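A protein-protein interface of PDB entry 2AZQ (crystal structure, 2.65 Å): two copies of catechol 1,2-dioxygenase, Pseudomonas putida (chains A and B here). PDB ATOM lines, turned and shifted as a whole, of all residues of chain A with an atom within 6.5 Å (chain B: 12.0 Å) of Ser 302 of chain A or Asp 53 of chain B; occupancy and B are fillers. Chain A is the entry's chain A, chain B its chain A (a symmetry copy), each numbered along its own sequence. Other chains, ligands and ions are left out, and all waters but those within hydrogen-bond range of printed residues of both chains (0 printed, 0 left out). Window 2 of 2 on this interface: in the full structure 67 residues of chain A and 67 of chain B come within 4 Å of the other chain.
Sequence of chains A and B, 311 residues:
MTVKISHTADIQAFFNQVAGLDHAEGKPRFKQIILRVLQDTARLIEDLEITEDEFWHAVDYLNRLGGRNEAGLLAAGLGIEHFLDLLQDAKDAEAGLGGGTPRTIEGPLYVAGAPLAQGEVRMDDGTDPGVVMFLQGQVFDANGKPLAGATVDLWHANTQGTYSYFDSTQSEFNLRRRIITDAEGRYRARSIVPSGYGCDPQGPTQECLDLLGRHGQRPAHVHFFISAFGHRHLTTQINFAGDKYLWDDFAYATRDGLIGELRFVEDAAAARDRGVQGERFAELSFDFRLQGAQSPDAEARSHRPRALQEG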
ATOM      1  N   GLU A 106       1.184  21.199 -29.121  1.00  0.00           N
ATOM      2  CA  GLU A 106       0.741  20.966 -27.746  1.00  0.00           C
ATOM      3  C   GLU A 106       0.091  22.194 -27.098  1.00  0.00           C
ATOM      4  O   GLU A 106      -0.951  22.080 -26.458  1.00  0.00           O
ATOM      5  CB  GLU A 106       1.938  20.533 -26.890  1.00  0.00           C
ATOM      6  CG  GLU A 106       1.684  20.551 -25.384  1.00  0.00           C
ATOM      7  CD  GLU A 106       2.884  20.063 -24.553  1.00  0.00           C
ATOM      8  OE1 GLU A 106       2.867  20.240 -23.321  1.00  0.00           O
ATOM      9  OE2 GLU A 106       3.838  19.499 -25.119  1.00  0.00           O
ATOM     10  N   HIS A 233       4.069   7.884 -28.341  1.00  0.00           N
ATOM     11  CA  HIS A 233       3.338   8.960 -27.706  1.00  0.00           C
ATOM     12  C   HIS A 233       2.867   9.962 -28.751  1.00  0.00           C
ATOM     13  O   HIS A 233       3.636  10.334 -29.642  1.00  0.00           O
ATOM     14  CB  HIS A 233       4.259   9.628 -26.698  1.00  0.00           C
ATOM     15  CG  HIS A 233       3.639  10.781 -25.972  1.00  0.00           C
ATOM     16  ND1 HIS A 233       3.193  10.686 -24.669  1.00  0.00           N
ATOM     17  CD2 HIS A 233       3.401  12.059 -26.365  1.00  0.00           C
ATOM     18  CE1 HIS A 233       2.710  11.857 -24.291  1.00  0.00           C
ATOM     19  NE2 HIS A 233       2.825  12.706 -25.302  1.00  0.00           N
ATOM     20  N   ALA A 300       7.146   9.117 -24.234  1.00  0.00           N
ATOM     21  CA  ALA A 300       7.930   9.764 -23.211  1.00  0.00           C
ATOM     22  C   ALA A 300       7.735  11.253 -23.115  1.00  0.00           C
ATOM     23  O   ALA A 300       8.376  11.905 -22.271  1.00  0.00           O
ATOM     24  CB  ALA A 300       9.412   9.442 -23.407  1.00  0.00           C
ATOM     25  N   ARG A 301       6.864  11.816 -23.943  1.00  0.00           N
ATOM     26  CA  ARG A 301       6.678  13.255 -23.850  1.00  0.00           C
ATOM     27  C   ARG A 301       8.036  13.952 -24.024  1.00  0.00           C
ATOM     28  O   ARG A 301       9.092  13.419 -23.667  1.00  0.00           O
ATOM     29  CB  ARG A 301       6.154  13.634 -22.458  1.00  0.00           C
ATOM     30  CG  ARG A 301       4.739  14.159 -22.357  1.00  0.00           C
ATOM     31  CD  ARG A 301       4.561  14.718 -20.952  1.00  0.00           C
ATOM     32  NE  ARG A 301       3.511  14.062 -20.187  1.00  0.00           N
ATOM     33  CZ  ARG A 301       3.316  14.261 -18.884  1.00  0.00           C
ATOM     34  NH1 ARG A 301       4.106  15.098 -18.204  1.00  0.00           N
ATOM     35  NH2 ARG A 301       2.321  13.635 -18.254  1.00  0.00           N
ATOM     36  N   SER A 302       8.004  15.160 -24.561  1.00  0.00           N
ATOM     37  CA  SER A 302       9.228  15.912 -24.710  1.00  0.00           C
ATOM     38  C   SER A 302       9.603  16.242 -23.269  1.00  0.00           C
ATOM     39  O   SER A 302       8.812  16.010 -22.348  1.00  0.00           O
ATOM     40  CB  SER A 302       8.953  17.206 -25.467  1.00  0.00           C
ATOM     41  OG  SER A 302       8.131  18.049 -24.693  1.00  0.00           O
ATOM     42  N   HIS A 303      10.807  16.760 -23.061  1.00  0.00           N
ATOM     43  CA  HIS A 303      11.186  17.158 -21.713  1.00  0.00           C
ATOM     44  C   HIS A 303      10.694  18.589 -21.555  1.00  0.00           C
ATOM     45  O   HIS A 303      11.082  19.289 -20.625  1.00  0.00           O
ATOM     46  CB  HIS A 303      12.708  17.132 -21.491  1.00  0.00           C
ATOM     47  CG  HIS A 303      13.358  15.826 -21.834  1.00  0.00           C
ATOM     48  ND1 HIS A 303      12.775  14.603 -21.561  1.00  0.00           N
ATOM     49  CD2 HIS A 303      14.558  15.550 -22.407  1.00  0.00           C
ATOM     50  CE1 HIS A 303      13.584  13.632 -21.955  1.00  0.00           C
ATOM     51  NE2 HIS A 303      14.672  14.181 -22.472  1.00  0.00           N
ATOM     52  N   ARG A 304       9.865  19.037 -22.490  1.00  0.00           N
ATOM     53  CA  ARG A 304       9.336  20.373 -22.379  1.00  0.00           C
ATOM     54  C   ARG A 304       8.834  20.564 -20.935  1.00  0.00           C
ATOM     55  O   ARG A 304       8.168  19.687 -20.378  1.00  0.00           O
ATOM     56  CB  ARG A 304       8.191  20.567 -23.373  1.00  0.00           C
ATOM     57  CG  ARG A 304       7.501  21.912 -23.252  1.00  0.00           C
ATOM     58  CD  ARG A 304       6.474  22.173 -24.344  1.00  0.00           C
ATOM     59  NE  ARG A 304       5.928  23.511 -24.167  1.00  0.00           N
ATOM     60  CZ  ARG A 304       5.108  24.118 -25.010  1.00  0.00           C
ATOM     61  NH1 ARG A 304       4.672  25.346 -24.748  1.00  0.00           N
ATOM     62  NH2 ARG A 304       4.723  23.506 -26.109  1.00  0.00           N
ATOM     63  N   PRO A 305       9.233  21.667 -20.282  1.00  0.00           N
ATOM     64  CA  PRO A 305       8.833  22.001 -18.911  1.00  0.00           C
ATOM     65  C   PRO A 305       7.314  22.271 -18.852  1.00  0.00           C
ATOM     66  O   PRO A 305       6.747  22.894 -19.753  1.00  0.00           O
ATOM     67  CB  PRO A 305       9.660  23.250 -18.626  1.00  0.00           C
ATOM     68  CG  PRO A 305      10.897  23.028 -19.479  1.00  0.00           C
ATOM     69  CD  PRO A 305      10.202  22.659 -20.771  1.00  0.00           C
ATOM     70  N   ARG A 306       6.640  21.804 -17.805  1.00  0.00           N
ATOM     71  CA  ARG A 306       5.205  22.010 -17.737  1.00  0.00           C
ATOM     72  C   ARG A 306       4.712  22.225 -16.335  1.00  0.00           C
ATOM     73  O   ARG A 306       5.294  21.739 -15.373  1.00  0.00           O
ATOM     74  CB  ARG A 306       4.479  20.819 -18.374  1.00  0.00           C
ATOM     75  CG  ARG A 306       4.820  20.645 -19.854  1.00  0.00           C
ATOM     76  CD  ARG A 306       4.314  19.327 -20.367  1.00  0.00           C
ATOM     77  NE  ARG A 306       4.777  19.009 -21.713  1.00  0.00           N
ATOM     78  CZ  ARG A 306       5.662  18.061 -21.999  1.00  0.00           C
ATOM     79  NH1 ARG A 306       6.198  17.324 -21.035  1.00  0.00           N
ATOM     80  NH2 ARG A 306       5.990  17.832 -23.254  1.00  0.00           N
ATOM     81  N   GLN A 309       4.975  19.392 -13.421  1.00  0.00           N
ATOM     82  CA  GLN A 309       5.594  18.079 -13.538  1.00  0.00           C
ATOM     83  C   GLN A 309       6.741  17.957 -12.540  1.00  0.00           C
ATOM     84  O   GLN A 309       7.310  16.881 -12.353  1.00  0.00           O
ATOM     85  CB  GLN A 309       6.021  17.723 -14.971  1.00  0.00           C
ATOM     86  CG  GLN A 309       6.811  18.712 -15.779  1.00  0.00           C
ATOM     87  CD  GLN A 309       7.118  18.129 -17.161  1.00  0.00           C
ATOM     88  OE1 GLN A 309       6.219  17.721 -17.891  1.00  0.00           O
ATOM     89  NE2 GLN A 309       8.393  18.077 -17.511  1.00  0.00           N
ATOM     90  N   ILE B  45      17.809  25.773 -36.426  1.00  0.00           N
ATOM     91  CA  ILE B  45      17.185  24.519 -36.089  1.00  0.00           C
ATOM     92  C   ILE B  45      17.532  23.435 -37.105  1.00  0.00           C
ATOM     93  O   ILE B  45      17.740  22.288 -36.742  1.00  0.00           O
ATOM     94  CB  ILE B  45      15.660  24.690 -35.992  1.00  0.00           C
ATOM     95  CG1 ILE B  45      15.335  25.659 -34.854  1.00  0.00           C
ATOM     96  CG2 ILE B  45      14.991  23.337 -35.801  1.00  0.00           C
ATOM     97  CD1 ILE B  45      13.903  26.158 -34.868  1.00  0.00           C
ATOM     98  N   LEU B  48      21.850  23.125 -37.052  1.00  0.00           N
ATOM     99  CA  LEU B  48      22.475  22.602 -35.840  1.00  0.00           C
ATOM    100  C   LEU B  48      21.639  21.486 -35.267  1.00  0.00           C
ATOM    101  O   LEU B  48      21.937  20.924 -34.197  1.00  0.00           O
ATOM    102  CB  LEU B  48      22.659  23.710 -34.811  1.00  0.00           C
ATOM    103  CG  LEU B  48      23.434  24.902 -35.361  1.00  0.00           C
ATOM    104  CD1 LEU B  48      23.800  25.828 -34.249  1.00  0.00           C
ATOM    105  CD2 LEU B  48      24.671  24.425 -36.057  1.00  0.00           C
ATOM    106  N   GLU B  49      20.593  21.156 -36.011  1.00  0.00           N
ATOM    107  CA  GLU B  49      19.686  20.107 -35.609  1.00  0.00           C
ATOM    108  C   GLU B  49      19.320  20.192 -34.141  1.00  0.00           C
ATOM    109  O   GLU B  49      19.601  19.278 -33.364  1.00  0.00           O
ATOM    110  CB  GLU B  49      20.279  18.732 -35.913  1.00  0.00           C
ATOM    111  CG  GLU B  49      19.344  17.627 -35.528  1.00  0.00           C
ATOM    112  CD  GLU B  49      19.920  16.272 -35.769  1.00  0.00           C
ATOM    113  OE1 GLU B  49      21.107  16.053 -35.417  1.00  0.00           O
ATOM    114  OE2 GLU B  49      19.168  15.413 -36.295  1.00  0.00           O
ATOM    115  N   ILE B  50      18.695  21.303 -33.768  1.00  0.00           N
ATOM    116  CA  ILE B  50      18.253  21.494 -32.399  1.00  0.00           C
ATOM    117  C   ILE B  50      17.104  20.506 -32.137  1.00  0.00           C
ATOM    118  O   ILE B  50      16.200  20.348 -32.951  1.00  0.00           O
ATOM    119  CB  ILE B  50      17.791  22.975 -32.162  1.00  0.00           C
ATOM    120  CG1 ILE B  50      19.006  23.896 -32.039  1.00  0.00           C
ATOM    121  CG2 ILE B  50      16.991  23.111 -30.872  1.00  0.00           C
ATOM    122  CD1 ILE B  50      19.798  24.044 -33.286  1.00  0.00           C
ATOM    123  N   THR B  51      17.165  19.829 -31.001  1.00  0.00           N
ATOM    124  CA  THR B  51      16.154  18.860 -30.604  1.00  0.00           C
ATOM    125  C   THR B  51      14.901  19.605 -30.088  1.00  0.00           C
ATOM    126  O   THR B  51      14.957  20.813 -29.865  1.00  0.00           O
ATOM    127  CB  THR B  51      16.709  17.968 -29.451  1.00  0.00           C
ATOM    128  OG1 THR B  51      16.579  18.646 -28.197  1.00  0.00           O
ATOM    129  CG2 THR B  51      18.213  17.703 -29.658  1.00  0.00           C
ATOM    130  N   GLU B  52      13.779  18.905 -29.907  1.00  0.00           N
ATOM    131  CA  GLU B  52      12.602  19.568 -29.347  1.00  0.00           C
ATOM    132  C   GLU B  52      12.909  20.002 -27.918  1.00  0.00           C
ATOM    133  O   GLU B  52      12.491  21.093 -27.510  1.00  0.00           O
ATOM    134  CB  GLU B  52      11.395  18.654 -29.256  1.00  0.00           C
ATOM    135  CG  GLU B  52      10.929  18.058 -30.542  1.00  0.00           C
ATOM    136  CD  GLU B  52       9.449  17.759 -30.473  1.00  0.00           C
ATOM    137  OE1 GLU B  52       9.011  17.150 -29.455  1.00  0.00           O
ATOM    138  OE2 GLU B  52       8.739  18.144 -31.435  1.00  0.00           O
ATOM    139  N   ASP B  53      13.612  19.145 -27.157  1.00  0.00           N
ATOM    140  CA  ASP B  53      13.964  19.471 -25.774  1.00  0.00           C
ATOM    141  C   ASP B  53      14.822  20.717 -25.694  1.00  0.00           C
ATOM    142  O   ASP B  53      14.664  21.525 -24.788  1.00  0.00           O
ATOM    143  CB  ASP B  53      14.735  18.349 -25.089  1.00  0.00           C
ATOM    144  CG  ASP B  53      13.976  17.055 -25.053  1.00  0.00           C
ATOM    145  OD1 ASP B  53      12.788  17.067 -24.664  1.00  0.00           O
ATOM    146  OD2 ASP B  53      14.577  16.012 -25.393  1.00  0.00           O
ATOM    147  N   GLU B  54      15.735  20.879 -26.639  1.00  0.00           N
ATOM    148  CA  GLU B  54      16.587  22.049 -26.593  1.00  0.00           C
ATOM    149  C   GLU B  54      15.721  23.273 -26.877  1.00  0.00           C
ATOM    150  O   GLU B  54      15.787  24.277 -26.175  1.00  0.00           O
ATOM    151  CB  GLU B  54      17.758  21.913 -27.595  1.00  0.00           C
ATOM    152  CG  GLU B  54      18.598  20.709 -27.302  1.00  0.00           C
ATOM    153  CD  GLU B  54      19.839  20.570 -28.157  1.00  0.00           C
ATOM    154  OE1 GLU B  54      19.721  20.451 -29.391  1.00  0.00           O
ATOM    155  OE2 GLU B  54      20.943  20.561 -27.576  1.00  0.00           O
ATOM    156  N   PHE B  55      14.886  23.156 -27.893  1.00  0.00           N
ATOM    157  CA  PHE B  55      14.019  24.247 -28.288  1.00  0.00           C
ATOM    158  C   PHE B  55      13.129  24.716 -27.166  1.00  0.00           C
ATOM    159  O   PHE B  55      12.999  25.929 -26.957  1.00  0.00           O
ATOM    160  CB  PHE B  55      13.127  23.854 -29.454  1.00  0.00           C
ATOM    161  CG  PHE B  55      12.247  24.953 -29.895  1.00  0.00           C
ATOM    162  CD1 PHE B  55      12.677  25.856 -30.835  1.00  0.00           C
ATOM    163  CD2 PHE B  55      11.012  25.157 -29.289  1.00  0.00           C
ATOM    164  CE1 PHE B  55      11.902  26.952 -31.172  1.00  0.00           C
ATOM    165  CE2 PHE B  55      10.231  26.254 -29.618  1.00  0.00           C
ATOM    166  CZ  PHE B  55      10.688  27.152 -30.567  1.00  0.00           C
ATOM    167  N   TRP B  56      12.507  23.768 -26.455  1.00  0.00           N
ATOM    168  CA  TRP B  56      11.604  24.140 -25.362  1.00  0.00           C
ATOM    169  C   TRP B  56      12.275  24.565 -24.046  1.00  0.00           C
ATOM    170  O   TRP B  56      11.657  25.262 -23.233  1.00  0.00           O
ATOM    171  CB  TRP B  56      10.530  23.059 -25.147  1.00  0.00           C
ATOM    172  CG  TRP B  56       9.585  22.936 -26.365  1.00  0.00           C
ATOM    173  CD1 TRP B  56       9.555  21.927 -27.288  1.00  0.00           C
ATOM    174  CD2 TRP B  56       8.612  23.908 -26.816  1.00  0.00           C
ATOM    175  NE1 TRP B  56       8.634  22.208 -28.276  1.00  0.00           N
ATOM    176  CE2 TRP B  56       8.044  23.414 -28.009  1.00  0.00           C
ATOM    177  CE3 TRP B  56       8.171  25.147 -26.323  1.00  0.00           C
ATOM    178  CZ2 TRP B  56       7.060  24.111 -28.714  1.00  0.00           C
ATOM    179  CZ3 TRP B  56       7.187  25.840 -27.034  1.00  0.00           C
ATOM    180  CH2 TRP B  56       6.645  25.318 -28.212  1.00  0.00           C
ATOM    181  N   HIS B  57      13.528  24.177 -23.822  1.00  0.00           N
ATOM    182  CA  HIS B  57      14.237  24.660 -22.632  1.00  0.00           C
ATOM    183  C   HIS B  57      14.634  26.132 -22.938  1.00  0.00           C
ATOM    184  O   HIS B  57      14.705  26.973 -22.030  1.00  0.00           O
ATOM    185  CB  HIS B  57      15.478  23.801 -22.345  1.00  0.00           C
ATOM    186  CG  HIS B  57      15.173  22.542 -21.598  1.00  0.00           C
ATOM    187  ND1 HIS B  57      15.092  22.494 -20.220  1.00  0.00           N
ATOM    188  CD2 HIS B  57      14.832  21.306 -22.032  1.00  0.00           C
ATOM    189  CE1 HIS B  57      14.715  21.286 -19.839  1.00  0.00           C
ATOM    190  NE2 HIS B  57      14.549  20.546 -20.920  1.00  0.00           N
ATOM    191  N   ALA B  58      14.871  26.436 -24.219  1.00  0.00           N
ATOM    192  CA  ALA B  58      15.224  27.794 -24.622  1.00  0.00           C
ATOM    193  C   ALA B  58      13.999  28.702 -24.416  1.00  0.00           C
ATOM    194  O   ALA B  58      14.104  29.796 -23.842  1.00  0.00           O
ATOM    195  CB  ALA B  58      15.650  27.820 -26.080  1.00  0.00           C
ATOM    196  N   VAL B  59      12.839  28.255 -24.896  1.00  0.00           N
ATOM    197  CA  VAL B  59      11.626  29.032 -24.717  1.00  0.00           C
ATOM    198  C   VAL B  59      11.397  29.269 -23.206  1.00  0.00           C
ATOM    199  O   VAL B  59      11.061  30.386 -22.782  1.00  0.00           O
ATOM    200  CB  VAL B  59      10.401  28.308 -25.341  1.00  0.00           C
ATOM    201  CG1 VAL B  59       9.113  29.026 -24.943  1.00  0.00           C
ATOM    202  CG2 VAL B  59      10.546  28.253 -26.877  1.00  0.00           C
ATOM    203  N   ASP B  60      11.596  28.228 -22.392  1.00  0.00           N
ATOM    204  CA  ASP B  60      11.416  28.372 -20.950  1.00  0.00           C
ATOM    205  C   ASP B  60      12.504  29.238 -20.287  1.00  0.00           C
ATOM    206  O   ASP B  60      12.214  30.028 -19.390  1.00  0.00           O
ATOM    207  CB  ASP B  60      11.320  26.996 -20.295  1.00  0.00           C
ATOM    208  CG  ASP B  60      11.264  27.079 -18.790  1.00  0.00           C
ATOM    209  OD1 ASP B  60      12.331  27.094 -18.142  1.00  0.00           O
ATOM    210  OD2 ASP B  60      10.148  27.163 -18.251  1.00  0.00           O
ATOM    211  N   TYR B  61      13.750  29.090 -20.717  1.00  0.00           N
ATOM    212  CA  TYR B  61      14.827  29.916 -20.191  1.00  0.00           C
ATOM    213  C   TYR B  61      14.412  31.361 -20.444  1.00  0.00           C
ATOM    214  O   TYR B  61      14.566  32.237 -19.598  1.00  0.00           O
ATOM    215  CB  TYR B  61      16.108  29.642 -20.960  1.00  0.00           C
ATOM    216  CG  TYR B  61      17.200  30.621 -20.665  1.00  0.00           C
ATOM    217  CD1 TYR B  61      17.947  30.542 -19.480  1.00  0.00           C
ATOM    218  CD2 TYR B  61      17.511  31.631 -21.576  1.00  0.00           C
ATOM    219  CE1 TYR B  61      18.995  31.453 -19.222  1.00  0.00           C
ATOM    220  CE2 TYR B  61      18.542  32.543 -21.334  1.00  0.00           C
ATOM    221  CZ  TYR B  61      19.277  32.449 -20.169  1.00  0.00           C
ATOM    222  OH  TYR B  61      20.299  33.337 -19.966  1.00  0.00           O
ATOM    223  N   LEU B  62      13.876  31.587 -21.637  1.00  0.00           N
ATOM    224  CA  LEU B  62      13.419  32.896 -22.078  1.00  0.00           C
ATOM    225  C   LEU B  62      12.327  33.476 -21.169  1.00  0.00           C
ATOM    226  O   LEU B  62      12.161  34.697 -21.078  1.00  0.00           O
ATOM    227  CB  LEU B  62      12.896  32.775 -23.492  1.00  0.00           C
ATOM    228  CG  LEU B  62      13.186  33.913 -24.451  1.00  0.00           C
ATOM    229  CD1 LEU B  62      14.675  33.932 -24.756  1.00  0.00           C
ATOM    230  CD2 LEU B  62      12.398  33.672 -25.736  1.00  0.00           C
ATOM    231  N   ARG B  64      12.213  32.769 -17.907  1.00  0.00           N
ATOM    232  CA  ARG B  64      12.911  33.119 -16.689  1.00  0.00           C
ATOM    233  C   ARG B  64      13.812  34.341 -16.892  1.00  0.00           C
ATOM    234  O   ARG B  64      13.938  35.167 -15.969  1.00  0.00           O
ATOM    235  CB  ARG B  64      13.670  31.892 -16.163  1.00  0.00           C
ATOM    236  CG  ARG B  64      12.682  30.743 -15.988  1.00  0.00           C
ATOM    237  CD  ARG B  64      13.210  29.434 -15.440  1.00  0.00           C
ATOM    238  NE  ARG B  64      14.189  28.749 -16.271  1.00  0.00           N
ATOM    239  CZ  ARG B  64      15.500  28.975 -16.245  1.00  0.00           C
ATOM    240  NH1 ARG B  64      16.014  29.885 -15.424  1.00  0.00           N
ATOM    241  NH2 ARG B  64      16.309  28.267 -17.026  1.00  0.00           N
ATOM    242  N   GLU B 207      23.545  31.533 -15.372  1.00  0.00           N
ATOM    243  CA  GLU B 207      23.414  30.133 -15.710  1.00  0.00           C
ATOM    244  C   GLU B 207      23.798  29.963 -17.162  1.00  0.00           C
ATOM    245  O   GLU B 207      24.348  28.917 -17.522  1.00  0.00           O
ATOM    246  CB  GLU B 207      22.020  29.569 -15.374  1.00  0.00           C
ATOM    247  CG  GLU B 207      21.046  29.422 -16.482  1.00  0.00           C
ATOM    248  CD  GLU B 207      19.675  28.977 -15.961  1.00  0.00           C
ATOM    249  OE1 GLU B 207      19.101  29.680 -15.088  1.00  0.00           O
ATOM    250  OE2 GLU B 207      19.158  27.936 -16.424  1.00  0.00           O
ATOM    251  N   LEU B 211      27.384  27.842 -18.751  1.00  0.00           N
ATOM    252  CA  LEU B 211      27.416  26.880 -19.840  1.00  0.00           C
ATOM    253  C   LEU B 211      28.413  27.314 -20.883  1.00  0.00           C
ATOM    254  O   LEU B 211      28.792  26.540 -21.752  1.00  0.00           O
ATOM    255  CB  LEU B 211      26.057  26.747 -20.497  1.00  0.00           C
ATOM    256  CG  LEU B 211      25.057  25.957 -19.673  1.00  0.00           C
ATOM    257  CD1 LEU B 211      23.665  26.111 -20.291  1.00  0.00           C
ATOM    258  CD2 LEU B 211      25.518  24.499 -19.613  1.00  0.00           C
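Among the printed residues, merely in contact across the chains: Arg 304 of chain A with Trp 56 of chain B, Ser 302 of chain A with Asp 53 of chain B, His 303 of chain A with His 57 of chain B, Pro 305 of chain A with Trp 56 of chain B, Pro 305 of chain A with Asp 60 of chain B and Ser 302 of chain A with Glu 52 of chain B.
No position is printed for both chains. Of the 7 pairs that touch across the chains among the printed residues, none has its exchanged pair printed and touching as well.
The side-chain amide nitrogen of Gln 309 of chain A sits at hydrogen-bond distance from the backbone carbonyl oxygen of Arg 304 of chain A (3.3 Å). The side-chain hydroxyl of Thr 51 of chain B sits at hydrogen-bond distance from the backbone NH of Asp 53 of chain B (3.2 Å). OD1 of Asp 60 of chain B lies within salt-bridge range of NE of Arg 64 of chain B (3.1 Å). OG of Ser 302 of chain A is in hydrogen-bond range of NH2 of Arg 306 of chain A (2.6 Å). The backbone carbonyl oxygen (O) of Arg 304 of chain A sits at hydrogen-bond distance from the guanidinium group (NH1) of Arg 306 of chain A. N of Arg 304 of chain A sits close to OG of Ser 302 of chain A (3.0 Å).
Of the printed residues of chain B, Ser 302 of chain A touches Glu 52 (3.99 Å) and Asp 53 (3.6 Å). Of chain A, only Ser 302 and His 303 come within 4 Å of Asp 53 of chain B. Ala 300 of chain A touches none of the printed residues of chain B. Of the printed residues of chain B, Pro 305 of chain A touches Trp 56 and Asp 60. Of the printed residues of chain A, Trp 56 of chain B touches Arg 304 (3.4 Å) and Pro 305 (3.9 Å). The nearest printed residue of chain A that does not touch Asp 60 of chain B is Arg 306 of chain A (6.4 Å).
The backbone NH (N) of His 303 of chain A sits at hydrogen-bond distance from the side-chain carboxylate (OD1) of Asp 53 of chain B, 2.6 Å away.
Of the 19 printed residues of chain B, 5 touch a printed residue of chain A. Hydrophobic or aromatic side chains of chain B that line the printed part of chain A: Trp 56 and His 57. Among the printed residues, 7 pairs touch across the chains. Among the printed residues, no Asp or Glu carboxylate lies within 4 Å of a Lys or Arg side-chain nitrogen of the other chain.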
